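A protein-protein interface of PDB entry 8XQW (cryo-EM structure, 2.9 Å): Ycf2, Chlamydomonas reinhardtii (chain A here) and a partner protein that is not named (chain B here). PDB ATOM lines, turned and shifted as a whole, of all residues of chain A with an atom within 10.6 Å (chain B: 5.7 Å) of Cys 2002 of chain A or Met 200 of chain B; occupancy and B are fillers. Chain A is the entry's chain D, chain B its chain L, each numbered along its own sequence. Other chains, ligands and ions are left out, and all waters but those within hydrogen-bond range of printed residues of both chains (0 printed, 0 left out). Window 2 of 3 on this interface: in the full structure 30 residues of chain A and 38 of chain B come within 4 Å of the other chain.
Among the printed residues, merely in contact across the chains: Ser 2006 of chain A with Leu 199 of chain B (3.4 Å), Leu 2008 of chain A with Glu 196 of chain B (3.6 Å), Leu 2008 of chain A with Leu 199 of chain B (3.7 Å), Tyr 2005 of chain A with Gly 203 of chain B (3.7 Å) and Cys 2002 of chain A with Glu 204 of chain B (3.8 Å).
The backbone carbonyl oxygen (O) of Gln 2003 of chain A sits at hydrogen-bond distance from the backbone NH (N) of Leu 2008 of chain A, at 3.4 Å. OG of Ser 2006 of chain A sits at hydrogen-bond distance from O of Cys 2002 of chain A, 3.2 Å away. The side-chain hydroxyl of Tyr 2005 of chain A sits at hydrogen-bond distance from the backbone carbonyl oxygen of Glu 2043 of chain A, 3.2 Å away. The side-chain amide oxygen (OE1) of Gln 2012 of chain A sits close to the backbone carbonyl oxygen (O) of Leu 2008 of chain A, at 3.2 Å. The backbone carbonyl oxygen (O) of Gln 2003 of chain A lies within hydrogen-bond range of the side-chain hydroxyl (OG) of Ser 2006 of chain A (3.2 Å). O of Ser 1999 of chain A lies within hydrogen-bond range of SG of Cys 2002 of chain A.
The side-chain sulfur of Met 200 of chain B lies within hydrogen-bond range of the side-chain sulfur of Cys 2002 of chain A (3.5 Å).
Of chain B, only Met 200 (3.5 Å) and Glu 204 (3.8 Å) come within 4 Å of Cys 2002 of chain A. Of the printed residues of chain B, Tyr 2005 of chain A touches Gly 203 (3.7 Å). Of the printed residues of chain B, Leu 2008 of chain A touches Glu 196 and Leu 199. Of the printed residues of chain A, Glu 196 of chain B touches Leu 2008 (3.6 Å). No residue of chain A comes within 4 Å of Asn 197 of chain B. Leu 199 of chain B touches just these residues of chain A: Ser 2006 and Leu 2008. Of chain A, only Cys 2002 (3.5 Å) comes within 4 Å of Met 200 of chain B. No residue of chain A comes within 4 Å of Ser 201 of chain B. Glu 204 of chain B touches just one residue of chain A: Cys 2002. The nearest printed residue of chain A that does not touch Glu 196 of chain B is Gln 2012 of chain A (4.9 Å).
Of the 12 printed residues of chain B, 5 touch a printed residue of chain A. Printed residues of chain B that touch a printed residue of chain A: Glu 196, Leu 199, Met 200, Gly 203 and Glu 204. Among the printed residues, no Asp or Glu carboxylate lies within 4 Å of a Lys or Arg side-chain nitrogen of the other chain.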
ATOM      1  N   PHE A1981       4.080  23.703   5.248  1.00  0.00           N
ATOM      2  CA  PHE A1981       5.011  23.806   4.135  1.00  0.00           C
ATOM      3  C   PHE A1981       4.578  23.011   2.928  1.00  0.00           C
ATOM      4  O   PHE A1981       5.260  23.054   1.907  1.00  0.00           O
ATOM      5  CB  PHE A1981       6.397  23.357   4.571  1.00  0.00           C
ATOM      6  CG  PHE A1981       7.142  24.392   5.328  1.00  0.00           C
ATOM      7  CD1 PHE A1981       7.205  25.679   4.870  1.00  0.00           C
ATOM      8  CD2 PHE A1981       7.764  24.083   6.510  1.00  0.00           C
ATOM      9  CE1 PHE A1981       7.882  26.630   5.565  1.00  0.00           C
ATOM     10  CE2 PHE A1981       8.439  25.035   7.209  1.00  0.00           C
ATOM     11  CZ  PHE A1981       8.498  26.310   6.733  1.00  0.00           C
ATOM     12  N   GLN A1994      16.628  27.406   1.978  1.00  0.00           N
ATOM     13  CA  GLN A1994      16.657  26.300   2.921  1.00  0.00           C
ATOM     14  C   GLN A1994      17.312  26.705   4.228  1.00  0.00           C
ATOM     15  O   GLN A1994      16.832  26.349   5.304  1.00  0.00           O
ATOM     16  CB  GLN A1994      17.371  25.103   2.306  1.00  0.00           C
ATOM     17  CG  GLN A1994      16.952  24.780   0.896  1.00  0.00           C
ATOM     18  CD  GLN A1994      15.602  24.124   0.810  1.00  0.00           C
ATOM     19  OE1 GLN A1994      15.070  23.931  -0.270  1.00  0.00           O
ATOM     20  NE2 GLN A1994      15.045  23.769   1.940  1.00  0.00           N
ATOM     21  N   GLN A1995      18.400  27.464   4.167  1.00  0.00           N
ATOM     22  CA  GLN A1995      19.130  27.729   5.403  1.00  0.00           C
ATOM     23  C   GLN A1995      18.439  28.744   6.298  1.00  0.00           C
ATOM     24  O   GLN A1995      18.288  28.462   7.497  1.00  0.00           O
ATOM     25  CB  GLN A1995      20.564  28.141   5.095  1.00  0.00           C
ATOM     26  CG  GLN A1995      21.280  28.607   6.320  1.00  0.00           C
ATOM     27  CD  GLN A1995      22.720  28.880   6.057  1.00  0.00           C
ATOM     28  OE1 GLN A1995      23.185  28.724   4.936  1.00  0.00           O
ATOM     29  NE2 GLN A1995      23.444  29.289   7.080  1.00  0.00           N
ATOM     30  N   PRO A1996      18.014  29.920   5.828  1.00  0.00           N
ATOM     31  CA  PRO A1996      17.329  30.839   6.754  1.00  0.00           C
ATOM     32  C   PRO A1996      16.051  30.267   7.343  1.00  0.00           C
ATOM     33  O   PRO A1996      15.857  30.304   8.568  1.00  0.00           O
ATOM     34  CB  PRO A1996      17.066  32.072   5.886  1.00  0.00           C
ATOM     35  CG  PRO A1996      17.281  31.647   4.514  1.00  0.00           C
ATOM     36  CD  PRO A1996      18.284  30.576   4.541  1.00  0.00           C
ATOM     37  N   ILE A1997      15.177  29.716   6.505  1.00  0.00           N
ATOM     38  CA  ILE A1997      13.930  29.152   7.000  1.00  0.00           C
ATOM     39  C   ILE A1997      14.195  27.958   7.905  1.00  0.00           C
ATOM     40  O   ILE A1997      13.555  27.802   8.950  1.00  0.00           O
ATOM     41  CB  ILE A1997      13.020  28.785   5.821  1.00  0.00           C
ATOM     42  CG1 ILE A1997      12.802  30.003   4.941  1.00  0.00           C
ATOM     43  CG2 ILE A1997      11.694  28.318   6.311  1.00  0.00           C
ATOM     44  CD1 ILE A1997      12.148  31.142   5.658  1.00  0.00           C
ATOM     45  N   GLY A1998      15.147  27.101   7.534  1.00  0.00           N
ATOM     46  CA  GLY A1998      15.446  25.952   8.363  1.00  0.00           C
ATOM     47  C   GLY A1998      16.004  26.330   9.713  1.00  0.00           C
ATOM     48  O   GLY A1998      15.647  25.724  10.727  1.00  0.00           O
ATOM     49  N   SER A1999      16.871  27.335   9.755  1.00  0.00           N
ATOM     50  CA  SER A1999      17.383  27.802  11.029  1.00  0.00           C
ATOM     51  C   SER A1999      16.264  28.344  11.897  1.00  0.00           C
ATOM     52  O   SER A1999      16.195  28.040  13.092  1.00  0.00           O
ATOM     53  CB  SER A1999      18.440  28.869  10.798  1.00  0.00           C
ATOM     54  OG  SER A1999      19.680  28.280  10.477  1.00  0.00           O
ATOM     55  N   LEU A2000      15.367  29.136  11.310  1.00  0.00           N
ATOM     56  CA  LEU A2000      14.252  29.670  12.085  1.00  0.00           C
ATOM     57  C   LEU A2000      13.398  28.557  12.669  1.00  0.00           C
ATOM     58  O   LEU A2000      12.972  28.632  13.826  1.00  0.00           O
ATOM     59  CB  LEU A2000      13.400  30.574  11.211  1.00  0.00           C
ATOM     60  CG  LEU A2000      13.788  32.035  11.234  1.00  0.00           C
ATOM     61  CD1 LEU A2000      13.075  32.750  10.125  1.00  0.00           C
ATOM     62  CD2 LEU A2000      13.418  32.599  12.569  1.00  0.00           C
ATOM     63  N   VAL A2001      13.142  27.511  11.891  1.00  0.00           N
ATOM     64  CA  VAL A2001      12.280  26.439  12.376  1.00  0.00           C
ATOM     65  C   VAL A2001      12.963  25.666  13.494  1.00  0.00           C
ATOM     66  O   VAL A2001      12.353  25.374  14.528  1.00  0.00           O
ATOM     67  CB  VAL A2001      11.866  25.516  11.221  1.00  0.00           C
ATOM     68  CG1 VAL A2001      11.140  24.331  11.759  1.00  0.00           C
ATOM     69  CG2 VAL A2001      10.986  26.253  10.278  1.00  0.00           C
ATOM     70  N   CYS A2002      14.240  25.322  13.315  1.00  0.00           N
ATOM     71  CA  CYS A2002      14.899  24.525  14.343  1.00  0.00           C
ATOM     72  C   CYS A2002      15.067  25.332  15.619  1.00  0.00           C
ATOM     73  O   CYS A2002      15.085  24.773  16.719  1.00  0.00           O
ATOM     74  CB  CYS A2002      16.251  24.004  13.864  1.00  0.00           C
ATOM     75  SG  CYS A2002      17.648  25.067  14.248  1.00  0.00           S
ATOM     76  N   GLN A2003      15.186  26.657  15.499  1.00  0.00           N
ATOM     77  CA  GLN A2003      15.240  27.491  16.693  1.00  0.00           C
ATOM     78  C   GLN A2003      13.899  27.538  17.395  1.00  0.00           C
ATOM     79  O   GLN A2003      13.836  27.428  18.619  1.00  0.00           O
ATOM     80  CB  GLN A2003      15.676  28.903  16.347  1.00  0.00           C
ATOM     81  CG  GLN A2003      17.144  29.087  16.208  1.00  0.00           C
ATOM     82  CD  GLN A2003      17.470  30.455  15.686  1.00  0.00           C
ATOM     83  OE1 GLN A2003      16.665  31.372  15.792  1.00  0.00           O
ATOM     84  NE2 GLN A2003      18.646  30.602  15.101  1.00  0.00           N
ATOM     85  N   ILE A2004      12.814  27.727  16.649  1.00  0.00           N
ATOM     86  CA  ILE A2004      11.508  27.834  17.290  1.00  0.00           C
ATOM     87  C   ILE A2004      11.132  26.530  17.970  1.00  0.00           C
ATOM     88  O   ILE A2004      10.525  26.527  19.042  1.00  0.00           O
ATOM     89  CB  ILE A2004      10.442  28.264  16.273  1.00  0.00           C
ATOM     90  CG1 ILE A2004      10.616  29.731  15.922  1.00  0.00           C
ATOM     91  CG2 ILE A2004       9.081  28.062  16.842  1.00  0.00           C
ATOM     92  CD1 ILE A2004       9.660  30.216  14.890  1.00  0.00           C
ATOM     93  N   TYR A2005      11.506  25.398  17.380  1.00  0.00           N
ATOM     94  CA  TYR A2005      11.118  24.134  17.991  1.00  0.00           C
ATOM     95  C   TYR A2005      11.945  23.813  19.226  1.00  0.00           C
ATOM     96  O   TYR A2005      11.449  23.151  20.140  1.00  0.00           O
ATOM     97  CB  TYR A2005      11.228  23.003  16.986  1.00  0.00           C
ATOM     98  CG  TYR A2005       9.910  22.650  16.392  1.00  0.00           C
ATOM     99  CD1 TYR A2005       8.935  22.061  17.152  1.00  0.00           C
ATOM    100  CD2 TYR A2005       9.629  22.932  15.082  1.00  0.00           C
ATOM    101  CE1 TYR A2005       7.731  21.745  16.620  1.00  0.00           C
ATOM    102  CE2 TYR A2005       8.430  22.623  14.547  1.00  0.00           C
ATOM    103  CZ  TYR A2005       7.483  22.030  15.316  1.00  0.00           C
ATOM    104  OH  TYR A2005       6.272  21.716  14.770  1.00  0.00           O
ATOM    105  N   SER A2006      13.191  24.254  19.274  1.00  0.00           N
ATOM    106  CA  SER A2006      14.036  23.941  20.413  1.00  0.00           C
ATOM    107  C   SER A2006      13.813  24.867  21.590  1.00  0.00           C
ATOM    108  O   SER A2006      14.536  24.759  22.577  1.00  0.00           O
ATOM    109  CB  SER A2006      15.499  23.993  20.007  1.00  0.00           C
ATOM    110  OG  SER A2006      15.887  25.319  19.746  1.00  0.00           O
ATOM    111  N   GLY A2007      12.844  25.769  21.519  1.00  0.00           N
ATOM    112  CA  GLY A2007      12.596  26.702  22.593  1.00  0.00           C
ATOM    113  C   GLY A2007      13.587  27.835  22.716  1.00  0.00           C
ATOM    114  O   GLY A2007      13.408  28.696  23.580  1.00  0.00           O
ATOM    115  N   LEU A2008      14.626  27.871  21.891  1.00  0.00           N
ATOM    116  CA  LEU A2008      15.661  28.891  21.989  1.00  0.00           C
ATOM    117  C   LEU A2008      15.296  30.185  21.291  1.00  0.00           C
ATOM    118  O   LEU A2008      16.139  31.073  21.203  1.00  0.00           O
ATOM    119  CB  LEU A2008      16.967  28.376  21.397  1.00  0.00           C
ATOM    120  CG  LEU A2008      17.534  27.113  22.010  1.00  0.00           C
ATOM    121  CD1 LEU A2008      18.776  26.709  21.281  1.00  0.00           C
ATOM    122  CD2 LEU A2008      17.832  27.384  23.449  1.00  0.00           C
ATOM    123  N   PHE A2009      14.082  30.314  20.784  1.00  0.00           N
ATOM    124  CA  PHE A2009      13.718  31.505  20.041  1.00  0.00           C
ATOM    125  C   PHE A2009      13.394  32.677  20.946  1.00  0.00           C
ATOM    126  O   PHE A2009      13.624  33.820  20.553  1.00  0.00           O
ATOM    127  CB  PHE A2009      12.528  31.196  19.143  1.00  0.00           C
ATOM    128  CG  PHE A2009      12.114  32.328  18.269  1.00  0.00           C
ATOM    129  CD1 PHE A2009      12.838  32.650  17.150  1.00  0.00           C
ATOM    130  CD2 PHE A2009      10.976  33.045  18.546  1.00  0.00           C
ATOM    131  CE1 PHE A2009      12.447  33.676  16.345  1.00  0.00           C
ATOM    132  CE2 PHE A2009      10.584  34.064  17.737  1.00  0.00           C
ATOM    133  CZ  PHE A2009      11.319  34.384  16.641  1.00  0.00           C
ATOM    134  N   ASN A2010      12.888  32.424  22.152  1.00  0.00           N
ATOM    135  CA  ASN A2010      12.480  33.502  23.041  1.00  0.00           C
ATOM    136  C   ASN A2010      13.650  34.235  23.669  1.00  0.00           C
ATOM    137  O   ASN A2010      13.423  35.136  24.478  1.00  0.00           O
ATOM    138  CB  ASN A2010      11.595  32.963  24.157  1.00  0.00           C
ATOM    139  CG  ASN A2010      10.596  31.951  23.670  1.00  0.00           C
ATOM    140  OD1 ASN A2010      10.944  31.001  22.979  1.00  0.00           O
ATOM    141  ND2 ASN A2010       9.342  32.136  24.047  1.00  0.00           N
ATOM    142  N   GLN A2012      16.754  34.838  21.638  1.00  0.00           N
ATOM    143  CA  GLN A2012      17.645  35.331  20.607  1.00  0.00           C
ATOM    144  C   GLN A2012      17.465  36.829  20.449  1.00  0.00           C
ATOM    145  O   GLN A2012      16.495  37.417  20.922  1.00  0.00           O
ATOM    146  CB  GLN A2012      17.382  34.632  19.277  1.00  0.00           C
ATOM    147  CG  GLN A2012      17.561  33.136  19.307  1.00  0.00           C
ATOM    148  CD  GLN A2012      18.952  32.720  19.715  1.00  0.00           C
ATOM    149  OE1 GLN A2012      19.132  31.916  20.627  1.00  0.00           O
ATOM    150  NE2 GLN A2012      19.952  33.268  19.041  1.00  0.00           N
ATOM    151  N   LYS A2015      15.697  40.049  14.762  1.00  0.00           N
ATOM    152  CA  LYS A2015      16.297  40.118  13.442  1.00  0.00           C
ATOM    153  C   LYS A2015      15.473  40.988  12.511  1.00  0.00           C
ATOM    154  O   LYS A2015      14.302  41.272  12.760  1.00  0.00           O
ATOM    155  CB  LYS A2015      16.417  38.731  12.821  1.00  0.00           C
ATOM    156  CG  LYS A2015      17.596  37.930  13.250  1.00  0.00           C
ATOM    157  CD  LYS A2015      17.829  36.830  12.246  1.00  0.00           C
ATOM    158  CE  LYS A2015      18.083  35.513  12.929  1.00  0.00           C
ATOM    159  NZ  LYS A2015      16.921  35.101  13.755  1.00  0.00           N
ATOM    160  N   LEU A2040       5.378  29.286   7.511  1.00  0.00           N
ATOM    161  CA  LEU A2040       6.339  29.196   8.604  1.00  0.00           C
ATOM    162  C   LEU A2040       5.662  29.355   9.958  1.00  0.00           C
ATOM    163  O   LEU A2040       6.050  28.705  10.931  1.00  0.00           O
ATOM    164  CB  LEU A2040       7.428  30.245   8.429  1.00  0.00           C
ATOM    165  CG  LEU A2040       8.290  30.533   9.648  1.00  0.00           C
ATOM    166  CD1 LEU A2040       9.233  29.407   9.871  1.00  0.00           C
ATOM    167  CD2 LEU A2040       9.044  31.801   9.445  1.00  0.00           C
ATOM    168  N   GLU A2043       3.415  25.978  10.491  1.00  0.00           N
ATOM    169  CA  GLU A2043       4.156  24.748  10.719  1.00  0.00           C
ATOM    170  C   GLU A2043       4.640  24.646  12.153  1.00  0.00           C
ATOM    171  O   GLU A2043       4.663  23.555  12.721  1.00  0.00           O
ATOM    172  CB  GLU A2043       5.337  24.670   9.759  1.00  0.00           C
ATOM    173  CG  GLU A2043       6.048  23.341   9.760  1.00  0.00           C
ATOM    174  CD  GLU A2043       5.520  22.403   8.698  1.00  0.00           C
ATOM    175  OE1 GLU A2043       6.101  21.318   8.503  1.00  0.00           O
ATOM    176  OE2 GLU A2043       4.518  22.747   8.056  1.00  0.00           O
ATOM    177  N   THR A2044       5.016  25.766  12.758  1.00  0.00           N
ATOM    178  CA  THR A2044       5.539  25.785  14.113  1.00  0.00           C
ATOM    179  C   THR A2044       4.497  26.150  15.155  1.00  0.00           C
ATOM    180  O   THR A2044       4.777  26.029  16.345  1.00  0.00           O
ATOM    181  CB  THR A2044       6.703  26.764  14.203  1.00  0.00           C
ATOM    182  OG1 THR A2044       6.299  28.018  13.659  1.00  0.00           O
ATOM    183  CG2 THR A2044       7.861  26.268  13.407  1.00  0.00           C
ATOM    184  N   MET A2046       3.024  29.163  15.869  1.00  0.00           N
ATOM    185  CA  MET A2046       3.243  30.433  16.531  1.00  0.00           C
ATOM    186  C   MET A2046       2.129  31.410  16.186  1.00  0.00           C
ATOM    187  O   MET A2046       1.119  31.052  15.584  1.00  0.00           O
ATOM    188  CB  MET A2046       4.609  30.992  16.158  1.00  0.00           C
ATOM    189  CG  MET A2046       5.712  30.370  16.939  1.00  0.00           C
ATOM    190  SD  MET A2046       6.796  31.630  17.575  1.00  0.00           S
ATOM    191  CE  MET A2046       6.906  32.632  16.113  1.00  0.00           C
ATOM    192  N   GLN B 193      28.562  24.696  23.676  1.00  0.00           N
ATOM    193  CA  GLN B 193      27.967  24.549  22.360  1.00  0.00           C
ATOM    194  C   GLN B 193      27.444  23.140  22.155  1.00  0.00           C
ATOM    195  O   GLN B 193      26.527  22.938  21.360  1.00  0.00           O
ATOM    196  CB  GLN B 193      28.993  24.908  21.286  1.00  0.00           C
ATOM    197  CG  GLN B 193      28.531  24.757  19.845  1.00  0.00           C
ATOM    198  CD  GLN B 193      27.338  25.624  19.503  1.00  0.00           C
ATOM    199  OE1 GLN B 193      26.452  25.211  18.763  1.00  0.00           O
ATOM    200  NE2 GLN B 193      27.311  26.830  20.037  1.00  0.00           N
ATOM    201  N   TYR B 195      25.724  21.352  24.302  1.00  0.00           N
ATOM    202  CA  TYR B 195      24.349  21.323  24.754  1.00  0.00           C
ATOM    203  C   TYR B 195      23.430  22.033  23.777  1.00  0.00           C
ATOM    204  O   TYR B 195      22.281  21.623  23.603  1.00  0.00           O
ATOM    205  CB  TYR B 195      24.251  21.942  26.135  1.00  0.00           C
ATOM    206  CG  TYR B 195      22.875  21.896  26.711  1.00  0.00           C
ATOM    207  CD1 TYR B 195      22.260  20.700  26.980  1.00  0.00           C
ATOM    208  CD2 TYR B 195      22.193  23.052  26.994  1.00  0.00           C
ATOM    209  CE1 TYR B 195      21.008  20.656  27.502  1.00  0.00           C
ATOM    210  CE2 TYR B 195      20.941  23.017  27.516  1.00  0.00           C
ATOM    211  CZ  TYR B 195      20.354  21.815  27.768  1.00  0.00           C
ATOM    212  OH  TYR B 195      19.095  21.781  28.296  1.00  0.00           O
ATOM    213  N   GLU B 196      23.917  23.069  23.103  1.00  0.00           N
ATOM    214  CA  GLU B 196      23.106  23.727  22.087  1.00  0.00           C
ATOM    215  C   GLU B 196      22.855  22.806  20.902  1.00  0.00           C
ATOM    216  O   GLU B 196      21.739  22.747  20.377  1.00  0.00           O
ATOM    217  CB  GLU B 196      23.790  25.003  21.629  1.00  0.00           C
ATOM    218  CG  GLU B 196      22.842  26.038  21.116  1.00  0.00           C
ATOM    219  CD  GLU B 196      22.378  26.975  22.203  1.00  0.00           C
ATOM    220  OE1 GLU B 196      22.396  26.571  23.383  1.00  0.00           O
ATOM    221  OE2 GLU B 196      22.001  28.119  21.881  1.00  0.00           O
ATOM    222  N   ASN B 197      23.889  22.101  20.448  1.00  0.00           N
ATOM    223  CA  ASN B 197      23.695  21.112  19.398  1.00  0.00           C
ATOM    224  C   ASN B 197      22.670  20.070  19.809  1.00  0.00           C
ATOM    225  O   ASN B 197      21.840  19.650  18.996  1.00  0.00           O
ATOM    226  CB  ASN B 197      25.009  20.430  19.062  1.00  0.00           C
ATOM    227  CG  ASN B 197      26.018  21.375  18.516  1.00  0.00           C
ATOM    228  OD1 ASN B 197      25.682  22.469  18.086  1.00  0.00           O
ATOM    229  ND2 ASN B 197      27.274  20.969  18.523  1.00  0.00           N
ATOM    230  N   PHE B 198      22.715  19.628  21.064  1.00  0.00           N
ATOM    231  CA  PHE B 198      21.720  18.666  21.512  1.00  0.00           C
ATOM    232  C   PHE B 198      20.324  19.259  21.456  1.00  0.00           C
ATOM    233  O   PHE B 198      19.384  18.612  20.989  1.00  0.00           O
ATOM    234  CB  PHE B 198      22.016  18.179  22.921  1.00  0.00           C
ATOM    235  CG  PHE B 198      20.922  17.349  23.491  1.00  0.00           C
ATOM    236  CD1 PHE B 198      20.737  16.057  23.069  1.00  0.00           C
ATOM    237  CD2 PHE B 198      20.051  17.866  24.417  1.00  0.00           C
ATOM    238  CE1 PHE B 198      19.726  15.305  23.569  1.00  0.00           C
ATOM    239  CE2 PHE B 198      19.037  17.114  24.912  1.00  0.00           C
ATOM    240  CZ  PHE B 198      18.881  15.832  24.492  1.00  0.00           C
ATOM    241  N   LEU B 199      20.162  20.484  21.940  1.00  0.00           N
ATOM    242  CA  LEU B 199      18.839  21.092  21.930  1.00  0.00           C
ATOM    243  C   LEU B 199      18.294  21.238  20.521  1.00  0.00           C
ATOM    244  O   LEU B 199      17.100  21.030  20.293  1.00  0.00           O
ATOM    245  CB  LEU B 199      18.886  22.447  22.613  1.00  0.00           C
ATOM    246  CG  LEU B 199      18.637  22.470  24.107  1.00  0.00           C
ATOM    247  CD1 LEU B 199      18.433  23.885  24.509  1.00  0.00           C
ATOM    248  CD2 LEU B 199      17.426  21.667  24.444  1.00  0.00           C
ATOM    249  N   MET B 200      19.145  21.568  19.556  1.00  0.00           N
ATOM    250  CA  MET B 200      18.658  21.732  18.193  1.00  0.00           C
ATOM    251  C   MET B 200      18.311  20.396  17.547  1.00  0.00           C
ATOM    252  O   MET B 200      17.307  20.290  16.832  1.00  0.00           O
ATOM    253  CB  MET B 200      19.688  22.479  17.363  1.00  0.00           C
ATOM    254  CG  MET B 200      19.631  23.970  17.557  1.00  0.00           C
ATOM    255  SD  MET B 200      20.530  24.866  16.296  1.00  0.00           S
ATOM    256  CE  MET B 200      22.164  24.182  16.506  1.00  0.00           C
ATOM    257  N   SER B 201      19.111  19.361  17.796  1.00  0.00           N
ATOM    258  CA  SER B 201      18.743  18.039  17.307  1.00  0.00           C
ATOM    259  C   SER B 201      17.431  17.560  17.906  1.00  0.00           C
ATOM    260  O   SER B 201      16.614  16.956  17.202  1.00  0.00           O
ATOM    261  CB  SER B 201      19.846  17.047  17.608  1.00  0.00           C
ATOM    262  OG  SER B 201      21.062  17.494  17.056  1.00  0.00           O
ATOM    263  N   GLU B 202      17.198  17.831  19.187  1.00  0.00           N
ATOM    264  CA  GLU B 202      15.917  17.471  19.780  1.00  0.00           C
ATOM    265  C   GLU B 202      14.781  18.257  19.156  1.00  0.00           C
ATOM    266  O   GLU B 202      13.675  17.738  19.002  1.00  0.00           O
ATOM    267  CB  GLU B 202      15.939  17.695  21.282  1.00  0.00           C
ATOM    268  CG  GLU B 202      16.602  16.595  22.032  1.00  0.00           C
ATOM    269  CD  GLU B 202      15.744  15.360  22.160  1.00  0.00           C
ATOM    270  OE1 GLU B 202      14.670  15.441  22.780  1.00  0.00           O
ATOM    271  OE2 GLU B 202      16.152  14.300  21.649  1.00  0.00           O
ATOM    272  N   GLY B 203      15.022  19.516  18.805  1.00  0.00           N
ATOM    273  CA  GLY B 203      14.001  20.272  18.105  1.00  0.00           C
ATOM    274  C   GLY B 203      13.601  19.634  16.791  1.00  0.00           C
ATOM    275  O   GLY B 203      12.416  19.515  16.479  1.00  0.00           O
ATOM    276  N   GLU B 204      14.584  19.209  16.008  1.00  0.00           N
ATOM    277  CA  GLU B 204      14.270  18.528  14.754  1.00  0.00           C
ATOM    278  C   GLU B 204      13.509  17.236  14.991  1.00  0.00           C
ATOM    279  O   GLU B 204      12.587  16.903  14.242  1.00  0.00           O
ATOM    280  CB  GLU B 204      15.541  18.230  13.984  1.00  0.00           C
ATOM    281  CG  GLU B 204      16.015  19.370  13.157  1.00  0.00           C
ATOM    282  CD  GLU B 204      17.510  19.520  13.215  1.00  0.00           C
ATOM    283  OE1 GLU B 204      17.982  20.665  13.347  1.00  0.00           O
ATOM    284  OE2 GLU B 204      18.212  18.493  13.131  1.00  0.00           O
ATOM    285  N   ARG B 205      13.902  16.475  16.010  1.00  0.00           N
ATOM    286  CA  ARG B 205      13.199  15.232  16.297  1.00  0.00           C
ATOM    287  C   ARG B 205      11.751  15.485  16.686  1.00  0.00           C
ATOM    288  O   ARG B 205      10.852  14.740  16.285  1.00  0.00           O
ATOM    289  CB  ARG B 205      13.925  14.470  17.390  1.00  0.00           C
ATOM    290  CG  ARG B 205      14.855  13.444  16.837  1.00  0.00           C
ATOM    291  CD  ARG B 205      15.341  12.528  17.900  1.00  0.00           C
ATOM    292  NE  ARG B 205      16.300  13.178  18.775  1.00  0.00           N
ATOM    293  CZ  ARG B 205      17.596  13.260  18.522  1.00  0.00           C
ATOM    294  NH1 ARG B 205      18.087  12.735  17.414  1.00  0.00           N
ATOM    295  NH2 ARG B 205      18.399  13.868  19.376  1.00  0.00           N
